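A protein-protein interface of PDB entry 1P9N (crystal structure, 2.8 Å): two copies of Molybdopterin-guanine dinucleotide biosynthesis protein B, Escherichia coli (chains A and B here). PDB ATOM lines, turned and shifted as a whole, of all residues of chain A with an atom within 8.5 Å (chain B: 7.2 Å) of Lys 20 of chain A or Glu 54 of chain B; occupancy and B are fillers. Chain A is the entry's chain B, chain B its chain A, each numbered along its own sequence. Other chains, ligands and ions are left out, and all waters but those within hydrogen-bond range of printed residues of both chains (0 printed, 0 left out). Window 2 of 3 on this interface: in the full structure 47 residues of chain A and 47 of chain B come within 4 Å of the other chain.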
ATOM      1  N   PHE A   7      -2.523  -2.658  -3.394  1.00  0.00           N
ATOM      2  CA  PHE A   7      -2.867  -1.236  -3.425  1.00  0.00           C
ATOM      3  C   PHE A   7      -4.224  -0.975  -4.070  1.00  0.00           C
ATOM      4  O   PHE A   7      -4.316  -0.392  -5.157  1.00  0.00           O
ATOM      5  CB  PHE A   7      -1.795  -0.416  -4.158  1.00  0.00           C
ATOM      6  CG  PHE A   7      -0.940   0.439  -3.245  1.00  0.00           C
ATOM      7  CD1 PHE A   7      -0.014  -0.145  -2.379  1.00  0.00           C
ATOM      8  CD2 PHE A   7      -1.069   1.827  -3.252  1.00  0.00           C
ATOM      9  CE1 PHE A   7       0.768   0.638  -1.536  1.00  0.00           C
ATOM     10  CE2 PHE A   7      -0.288   2.625  -2.408  1.00  0.00           C
ATOM     11  CZ  PHE A   7       0.633   2.026  -1.548  1.00  0.00           C
ATOM     12  N   THR A  13      -8.362   6.666 -12.013  1.00  0.00           N
ATOM     13  CA  THR A  13      -6.902   6.674 -12.166  1.00  0.00           C
ATOM     14  C   THR A  13      -6.072   6.815 -10.888  1.00  0.00           C
ATOM     15  O   THR A  13      -5.214   5.979 -10.619  1.00  0.00           O
ATOM     16  CB  THR A  13      -6.465   7.792 -13.102  1.00  0.00           C
ATOM     17  OG1 THR A  13      -5.457   8.581 -12.456  1.00  0.00           O
ATOM     18  CG2 THR A  13      -7.657   8.675 -13.458  1.00  0.00           C
ATOM     19  N   GLY A  14      -6.317   7.880 -10.126  1.00  0.00           N
ATOM     20  CA  GLY A  14      -5.608   8.124  -8.877  1.00  0.00           C
ATOM     21  C   GLY A  14      -4.367   7.311  -8.515  1.00  0.00           C
ATOM     22  O   GLY A  14      -3.244   7.800  -8.658  1.00  0.00           O
ATOM     23  N   LYS A  15      -4.563   6.088  -8.022  1.00  0.00           N
ATOM     24  CA  LYS A  15      -3.452   5.234  -7.616  1.00  0.00           C
ATOM     25  C   LYS A  15      -2.246   5.244  -8.560  1.00  0.00           C
ATOM     26  O   LYS A  15      -1.138   4.893  -8.155  1.00  0.00           O
ATOM     27  CB  LYS A  15      -3.942   3.798  -7.377  1.00  0.00           C
ATOM     28  CG  LYS A  15      -4.583   3.104  -8.561  1.00  0.00           C
ATOM     29  CD  LYS A  15      -5.016   1.696  -8.152  1.00  0.00           C
ATOM     30  CE  LYS A  15      -5.723   0.943  -9.268  1.00  0.00           C
ATOM     31  NZ  LYS A  15      -7.080   1.473  -9.561  1.00  0.00           N
ATOM     32  N   THR A  16      -2.449   5.642  -9.813  1.00  0.00           N
ATOM     33  CA  THR A  16      -1.329   5.708 -10.755  1.00  0.00           C
ATOM     34  C   THR A  16      -0.632   7.057 -10.574  1.00  0.00           C
ATOM     35  O   THR A  16       0.581   7.174 -10.754  1.00  0.00           O
ATOM     36  CB  THR A  16      -1.795   5.533 -12.240  1.00  0.00           C
ATOM     37  OG1 THR A  16      -2.230   4.182 -12.446  1.00  0.00           O
ATOM     38  CG2 THR A  16      -0.652   5.828 -13.214  1.00  0.00           C
ATOM     39  N   THR A  17      -1.408   8.070 -10.204  1.00  0.00           N
ATOM     40  CA  THR A  17      -0.866   9.402  -9.966  1.00  0.00           C
ATOM     41  C   THR A  17      -0.252   9.382  -8.560  1.00  0.00           C
ATOM     42  O   THR A  17       0.720  10.085  -8.274  1.00  0.00           O
ATOM     43  CB  THR A  17      -1.973  10.458 -10.037  1.00  0.00           C
ATOM     44  OG1 THR A  17      -2.920  10.080 -11.046  1.00  0.00           O
ATOM     45  CG2 THR A  17      -1.382  11.818 -10.395  1.00  0.00           C
ATOM     46  N   LEU A  18      -0.837   8.556  -7.695  1.00  0.00           N
ATOM     47  CA  LEU A  18      -0.366   8.373  -6.329  1.00  0.00           C
ATOM     48  C   LEU A  18       0.968   7.635  -6.423  1.00  0.00           C
ATOM     49  O   LEU A  18       2.033   8.214  -6.171  1.00  0.00           O
ATOM     50  CB  LEU A  18      -1.392   7.542  -5.530  1.00  0.00           C
ATOM     51  CG  LEU A  18      -1.147   6.919  -4.138  1.00  0.00           C
ATOM     52  CD1 LEU A  18      -0.975   5.416  -4.257  1.00  0.00           C
ATOM     53  CD2 LEU A  18       0.061   7.536  -3.478  1.00  0.00           C
ATOM     54  N   LEU A  19       0.903   6.361  -6.803  1.00  0.00           N
ATOM     55  CA  LEU A  19       2.096   5.538  -6.933  1.00  0.00           C
ATOM     56  C   LEU A  19       3.207   6.249  -7.687  1.00  0.00           C
ATOM     57  O   LEU A  19       4.378   6.096  -7.357  1.00  0.00           O
ATOM     58  CB  LEU A  19       1.749   4.228  -7.625  1.00  0.00           C
ATOM     59  CG  LEU A  19       0.928   3.278  -6.760  1.00  0.00           C
ATOM     60  CD1 LEU A  19       0.378   2.158  -7.614  1.00  0.00           C
ATOM     61  CD2 LEU A  19       1.788   2.729  -5.646  1.00  0.00           C
ATOM     62  N   LYS A  20       2.845   7.034  -8.695  1.00  0.00           N
ATOM     63  CA  LYS A  20       3.838   7.768  -9.469  1.00  0.00           C
ATOM     64  C   LYS A  20       4.759   8.551  -8.537  1.00  0.00           C
ATOM     65  O   LYS A  20       5.893   8.880  -8.894  1.00  0.00           O
ATOM     66  CB  LYS A  20       3.152   8.747 -10.428  1.00  0.00           C
ATOM     67  CG  LYS A  20       4.120   9.714 -11.117  1.00  0.00           C
ATOM     68  CD  LYS A  20       3.444  11.039 -11.485  1.00  0.00           C
ATOM     69  CE  LYS A  20       2.664  10.966 -12.793  1.00  0.00           C
ATOM     70  NZ  LYS A  20       3.560  10.961 -13.986  1.00  0.00           N
ATOM     71  N   LYS A  21       4.264   8.840  -7.338  1.00  0.00           N
ATOM     72  CA  LYS A  21       5.026   9.607  -6.360  1.00  0.00           C
ATOM     73  C   LYS A  21       5.533   8.773  -5.190  1.00  0.00           C
ATOM     74  O   LYS A  21       6.547   9.105  -4.589  1.00  0.00           O
ATOM     75  CB  LYS A  21       4.169  10.761  -5.838  1.00  0.00           C
ATOM     76  CG  LYS A  21       3.591  11.643  -6.934  1.00  0.00           C
ATOM     77  CD  LYS A  21       2.714  12.736  -6.350  1.00  0.00           C
ATOM     78  CE  LYS A  21       2.035  13.559  -7.434  1.00  0.00           C
ATOM     79  NZ  LYS A  21       1.047  12.761  -8.220  1.00  0.00           N
ATOM     80  N   LEU A  22       4.829   7.695  -4.868  1.00  0.00           N
ATOM     81  CA  LEU A  22       5.239   6.838  -3.759  1.00  0.00           C
ATOM     82  C   LEU A  22       6.470   5.992  -4.115  1.00  0.00           C
ATOM     83  O   LEU A  22       7.258   5.621  -3.243  1.00  0.00           O
ATOM     84  CB  LEU A  22       4.090   5.907  -3.357  1.00  0.00           C
ATOM     85  CG  LEU A  22       4.075   5.366  -1.918  1.00  0.00           C
ATOM     86  CD1 LEU A  22       3.320   4.044  -1.881  1.00  0.00           C
ATOM     87  CD2 LEU A  22       5.474   5.145  -1.394  1.00  0.00           C
ATOM     88  N   ILE A  23       6.635   5.679  -5.396  1.00  0.00           N
ATOM     89  CA  ILE A  23       7.765   4.860  -5.821  1.00  0.00           C
ATOM     90  C   ILE A  23       9.093   5.530  -5.478  1.00  0.00           C
ATOM     91  O   ILE A  23       9.872   5.006  -4.681  1.00  0.00           O
ATOM     92  CB  ILE A  23       7.717   4.547  -7.360  1.00  0.00           C
ATOM     93  CG1 ILE A  23       6.527   3.641  -7.683  1.00  0.00           C
ATOM     94  CG2 ILE A  23       9.006   3.862  -7.796  1.00  0.00           C
ATOM     95  CD1 ILE A  23       6.608   2.282  -7.033  1.00  0.00           C
ATOM     96  N   PRO A  24       9.359   6.710  -6.063  1.00  0.00           N
ATOM     97  CA  PRO A  24      10.618   7.413  -5.783  1.00  0.00           C
ATOM     98  C   PRO A  24      10.843   7.533  -4.266  1.00  0.00           C
ATOM     99  O   PRO A  24      11.919   7.190  -3.746  1.00  0.00           O
ATOM    100  CB  PRO A  24      10.413   8.775  -6.450  1.00  0.00           C
ATOM    101  CG  PRO A  24       9.394   8.493  -7.529  1.00  0.00           C
ATOM    102  CD  PRO A  24       8.441   7.563  -6.839  1.00  0.00           C
ATOM    103  N   ALA A  25       9.809   8.016  -3.573  1.00  0.00           N
ATOM    104  CA  ALA A  25       9.851   8.175  -2.134  1.00  0.00           C
ATOM    105  C   ALA A  25      10.345   6.883  -1.517  1.00  0.00           C
ATOM    106  O   ALA A  25      11.076   6.904  -0.542  1.00  0.00           O
ATOM    107  CB  ALA A  25       8.473   8.516  -1.595  1.00  0.00           C
ATOM    108  N   LEU A  35       6.881  -3.987  -9.260  1.00  0.00           N
ATOM    109  CA  LEU A  35       5.449  -3.809  -9.434  1.00  0.00           C
ATOM    110  C   LEU A  35       4.720  -4.775 -10.391  1.00  0.00           C
ATOM    111  O   LEU A  35       4.828  -4.661 -11.618  1.00  0.00           O
ATOM    112  CB  LEU A  35       5.206  -2.364  -9.858  1.00  0.00           C
ATOM    113  CG  LEU A  35       3.774  -1.900 -10.095  1.00  0.00           C
ATOM    114  CD1 LEU A  35       3.498  -1.915 -11.573  1.00  0.00           C
ATOM    115  CD2 LEU A  35       2.786  -2.764  -9.304  1.00  0.00           C
ATOM    116  N   LEU A 101       5.298  -4.405  -5.164  1.00  0.00           N
ATOM    117  CA  LEU A 101       3.979  -3.788  -5.112  1.00  0.00           C
ATOM    118  C   LEU A 101       3.021  -4.595  -5.995  1.00  0.00           C
ATOM    119  O   LEU A 101       3.349  -4.910  -7.141  1.00  0.00           O
ATOM    120  CB  LEU A 101       4.033  -2.348  -5.626  1.00  0.00           C
ATOM    121  CG  LEU A 101       4.935  -1.349  -4.910  1.00  0.00           C
ATOM    122  CD1 LEU A 101       4.620   0.014  -5.463  1.00  0.00           C
ATOM    123  CD2 LEU A 101       4.707  -1.365  -3.417  1.00  0.00           C
ATOM    124  N   GLU A 103      -0.703  -4.503  -7.683  1.00  0.00           N
ATOM    125  CA  GLU A 103      -1.919  -3.773  -8.028  1.00  0.00           C
ATOM    126  C   GLU A 103      -2.757  -4.511  -9.067  1.00  0.00           C
ATOM    127  O   GLU A 103      -2.206  -5.135  -9.974  1.00  0.00           O
ATOM    128  CB  GLU A 103      -1.552  -2.398  -8.571  1.00  0.00           C
ATOM    129  CG  GLU A 103      -2.431  -1.922  -9.701  1.00  0.00           C
ATOM    130  CD  GLU A 103      -2.026  -0.564 -10.207  1.00  0.00           C
ATOM    131  OE1 GLU A 103      -0.815  -0.318 -10.355  1.00  0.00           O
ATOM    132  OE2 GLU A 103      -2.918   0.259 -10.467  1.00  0.00           O
ATOM    133  N   VAL A 154       2.855  11.798   0.693  1.00  0.00           N
ATOM    134  CA  VAL A 154       3.570  10.660   0.143  1.00  0.00           C
ATOM    135  C   VAL A 154       4.624  10.221   1.151  1.00  0.00           C
ATOM    136  O   VAL A 154       4.764   9.030   1.457  1.00  0.00           O
ATOM    137  CB  VAL A 154       4.256  11.042  -1.165  1.00  0.00           C
ATOM    138  CG1 VAL A 154       3.238  11.128  -2.267  1.00  0.00           C
ATOM    139  CG2 VAL A 154       4.945  12.390  -1.004  1.00  0.00           C
ATOM    140  N   ASP B  51       1.735   2.262 -21.292  1.00  0.00           N
ATOM    141  CA  ASP B  51       1.557   0.900 -20.787  1.00  0.00           C
ATOM    142  C   ASP B  51       2.256   0.776 -19.444  1.00  0.00           C
ATOM    143  O   ASP B  51       3.179  -0.018 -19.297  1.00  0.00           O
ATOM    144  CB  ASP B  51       2.144  -0.115 -21.781  1.00  0.00           C
ATOM    145  CG  ASP B  51       2.117  -1.573 -21.260  1.00  0.00           C
ATOM    146  OD1 ASP B  51       1.045  -2.089 -20.875  1.00  0.00           O
ATOM    147  OD2 ASP B  51       3.186  -2.237 -21.244  1.00  0.00           O
ATOM    148  N   SER B  52       1.816   1.565 -18.465  1.00  0.00           N
ATOM    149  CA  SER B  52       2.406   1.532 -17.121  1.00  0.00           C
ATOM    150  C   SER B  52       3.849   2.031 -17.257  1.00  0.00           C
ATOM    151  O   SER B  52       4.751   1.592 -16.544  1.00  0.00           O
ATOM    152  CB  SER B  52       2.378   0.096 -16.570  1.00  0.00           C
ATOM    153  OG  SER B  52       2.453   0.068 -15.151  1.00  0.00           O
ATOM    154  N   TYR B  53       4.032   2.962 -18.192  1.00  0.00           N
ATOM    155  CA  TYR B  53       5.320   3.564 -18.498  1.00  0.00           C
ATOM    156  C   TYR B  53       5.768   4.488 -17.393  1.00  0.00           C
ATOM    157  O   TYR B  53       6.942   4.501 -17.005  1.00  0.00           O
ATOM    158  CB  TYR B  53       5.218   4.348 -19.812  1.00  0.00           C
ATOM    159  CG  TYR B  53       6.382   5.274 -20.111  1.00  0.00           C
ATOM    160  CD1 TYR B  53       7.670   4.777 -20.278  1.00  0.00           C
ATOM    161  CD2 TYR B  53       6.191   6.655 -20.231  1.00  0.00           C
ATOM    162  CE1 TYR B  53       8.747   5.627 -20.558  1.00  0.00           C
ATOM    163  CE2 TYR B  53       7.270   7.521 -20.512  1.00  0.00           C
ATOM    164  CZ  TYR B  53       8.545   6.992 -20.673  1.00  0.00           C
ATOM    165  OH  TYR B  53       9.622   7.808 -20.948  1.00  0.00           O
ATOM    166  N   GLU B  54       4.816   5.262 -16.885  1.00  0.00           N
ATOM    167  CA  GLU B  54       5.081   6.229 -15.827  1.00  0.00           C
ATOM    168  C   GLU B  54       5.722   5.614 -14.581  1.00  0.00           C
ATOM    169  O   GLU B  54       6.751   6.089 -14.110  1.00  0.00           O
ATOM    170  CB  GLU B  54       3.777   6.941 -15.437  1.00  0.00           C
ATOM    171  CG  GLU B  54       3.011   7.617 -16.586  1.00  0.00           C
ATOM    172  CD  GLU B  54       3.888   8.500 -17.467  1.00  0.00           C
ATOM    173  OE1 GLU B  54       4.499   9.466 -16.960  1.00  0.00           O
ATOM    174  OE2 GLU B  54       3.961   8.220 -18.683  1.00  0.00           O
ATOM    175  N   LEU B  55       5.116   4.555 -14.054  1.00  0.00           N
ATOM    176  CA  LEU B  55       5.627   3.908 -12.853  1.00  0.00           C
ATOM    177  C   LEU B  55       6.966   3.217 -13.041  1.00  0.00           C
ATOM    178  O   LEU B  55       7.584   2.784 -12.075  1.00  0.00           O
ATOM    179  CB  LEU B  55       4.618   2.889 -12.338  1.00  0.00           C
ATOM    180  CG  LEU B  55       3.194   3.386 -12.099  1.00  0.00           C
ATOM    181  CD1 LEU B  55       2.534   3.744 -13.422  1.00  0.00           C
ATOM    182  CD2 LEU B  55       2.406   2.300 -11.397  1.00  0.00           C
ATOM    183  N   ARG B  56       7.419   3.101 -14.280  1.00  0.00           N
ATOM    184  CA  ARG B  56       8.687   2.431 -14.528  1.00  0.00           C
ATOM    185  C   ARG B  56       9.814   3.448 -14.520  1.00  0.00           C
ATOM    186  O   ARG B  56      10.791   3.298 -13.780  1.00  0.00           O
ATOM    187  CB  ARG B  56       8.653   1.694 -15.867  1.00  0.00           C
ATOM    188  CG  ARG B  56       9.486   0.406 -15.893  1.00  0.00           C
ATOM    189  CD  ARG B  56       9.404  -0.257 -17.255  1.00  0.00           C
ATOM    190  NE  ARG B  56       8.036  -0.211 -17.758  1.00  0.00           N
ATOM    191  CZ  ARG B  56       7.705   0.161 -18.989  1.00  0.00           C
ATOM    192  NH1 ARG B  56       8.645   0.517 -19.859  1.00  0.00           N
ATOM    193  NH2 ARG B  56       6.429   0.196 -19.345  1.00  0.00           N
ATOM    194  N   LYS B  57       9.681   4.481 -15.344  1.00  0.00           N
ATOM    195  CA  LYS B  57      10.696   5.523 -15.388  1.00  0.00           C
ATOM    196  C   LYS B  57      10.618   6.280 -14.074  1.00  0.00           C
ATOM    197  O   LYS B  57      11.468   7.114 -13.786  1.00  0.00           O
ATOM    198  CB  LYS B  57      10.456   6.480 -16.560  1.00  0.00           C
ATOM    199  CG  LYS B  57      10.595   5.835 -17.937  1.00  0.00           C
ATOM    200  CD  LYS B  57      12.020   5.362 -18.247  1.00  0.00           C
ATOM    201  CE  LYS B  57      12.939   6.505 -18.672  1.00  0.00           C
ATOM    202  NZ  LYS B  57      13.195   7.475 -17.569  1.00  0.00           N
ATOM    203  N   ALA B  58       9.591   5.973 -13.280  1.00  0.00           N
ATOM    204  CA  ALA B  58       9.389   6.603 -11.983  1.00  0.00           C
ATOM    205  C   ALA B  58      10.238   5.923 -10.916  1.00  0.00           C
ATOM    206  O   ALA B  58      10.636   6.560  -9.942  1.00  0.00           O
ATOM    207  CB  ALA B  58       7.924   6.551 -11.593  1.00  0.00           C
ATOM    208  N   GLY B  59      10.514   4.631 -11.091  1.00  0.00           N
ATOM    209  CA  GLY B  59      11.340   3.933 -10.119  1.00  0.00           C
ATOM    210  C   GLY B  59      11.106   2.445  -9.941  1.00  0.00           C
ATOM    211  O   GLY B  59      11.724   1.815  -9.077  1.00  0.00           O
ATOM    212  N   ALA B  60      10.211   1.877 -10.744  1.00  0.00           N
ATOM    213  CA  ALA B  60       9.916   0.445 -10.664  1.00  0.00           C
ATOM    214  C   ALA B  60      10.842  -0.287 -11.630  1.00  0.00           C
ATOM    215  O   ALA B  60      10.482  -0.556 -12.776  1.00  0.00           O
ATOM    216  CB  ALA B  60       8.471   0.192 -11.031  1.00  0.00           C
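NZ of Lys 20 of chain A is in salt-bridge range of OE1 of Glu 54 of chain B.
The backbone carbonyl oxygen (O) of Leu 55 of chain B lies close to the backbone NH (N) of Ala 60 of chain B (3.1 Å).
CD1 of Leu 55 of chain B touches CG2 of Thr 16 of chain A, 3.8 Å away.
O of Ala 58 of chain B touches CG2 of Ile 23 of chain A, at 3.8 Å.
Ile 23 of chain A touches Gly 59 of chain B (CG2 to CA, 3.3 Å).
Ala 60 of chain B touches Ile 23 of chain A (N to CG2, 3.8 Å).
Pro 24 of chain A touches Ala 58 of chain B.
Of chain B, only Glu 54 comes within 4 Å of Lys 20 of chain A.
Of chain A, only Lys 20 comes within 4 Å of Glu 54 of chain B.
Of the printed residues of chain B, Thr 16 of chain A touches Leu 55 (3.8 Å).
Printed residues of chain A within 4 Å of Leu 55 of chain B: Thr 16 (3.8 Å).
Printed residues of chain A within 4 Å of Ala 58 of chain B: Ile 23 and Pro 24.
Of the printed residues of chain A, Ala 60 of chain B touches Ile 23 (3.8 Å).
Printed residues of chain B within 4 Å of Pro 24 of chain A: Ala 58.
Phe 7 of chain A touches none of the printed residues of chain B.
Lys 15 of chain A touches none of the printed residues of chain B.
Hydrophobic or aromatic side chains of chain B that line the printed part of chain A: Leu 55.
Along chain B the printed residues that touch a printed residue of chain A span positions 54 to 60.
Among the printed residues, Asp or Glu carboxylates within 4 Å of a Lys or Arg side-chain nitrogen of the other chain: Lys 20 of chain A with Glu 54 of chain B.
No position is printed for both chains.
Of the 6 pairs that touch across the chains among the printed residues, none has its exchanged pair printed and touching as well.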
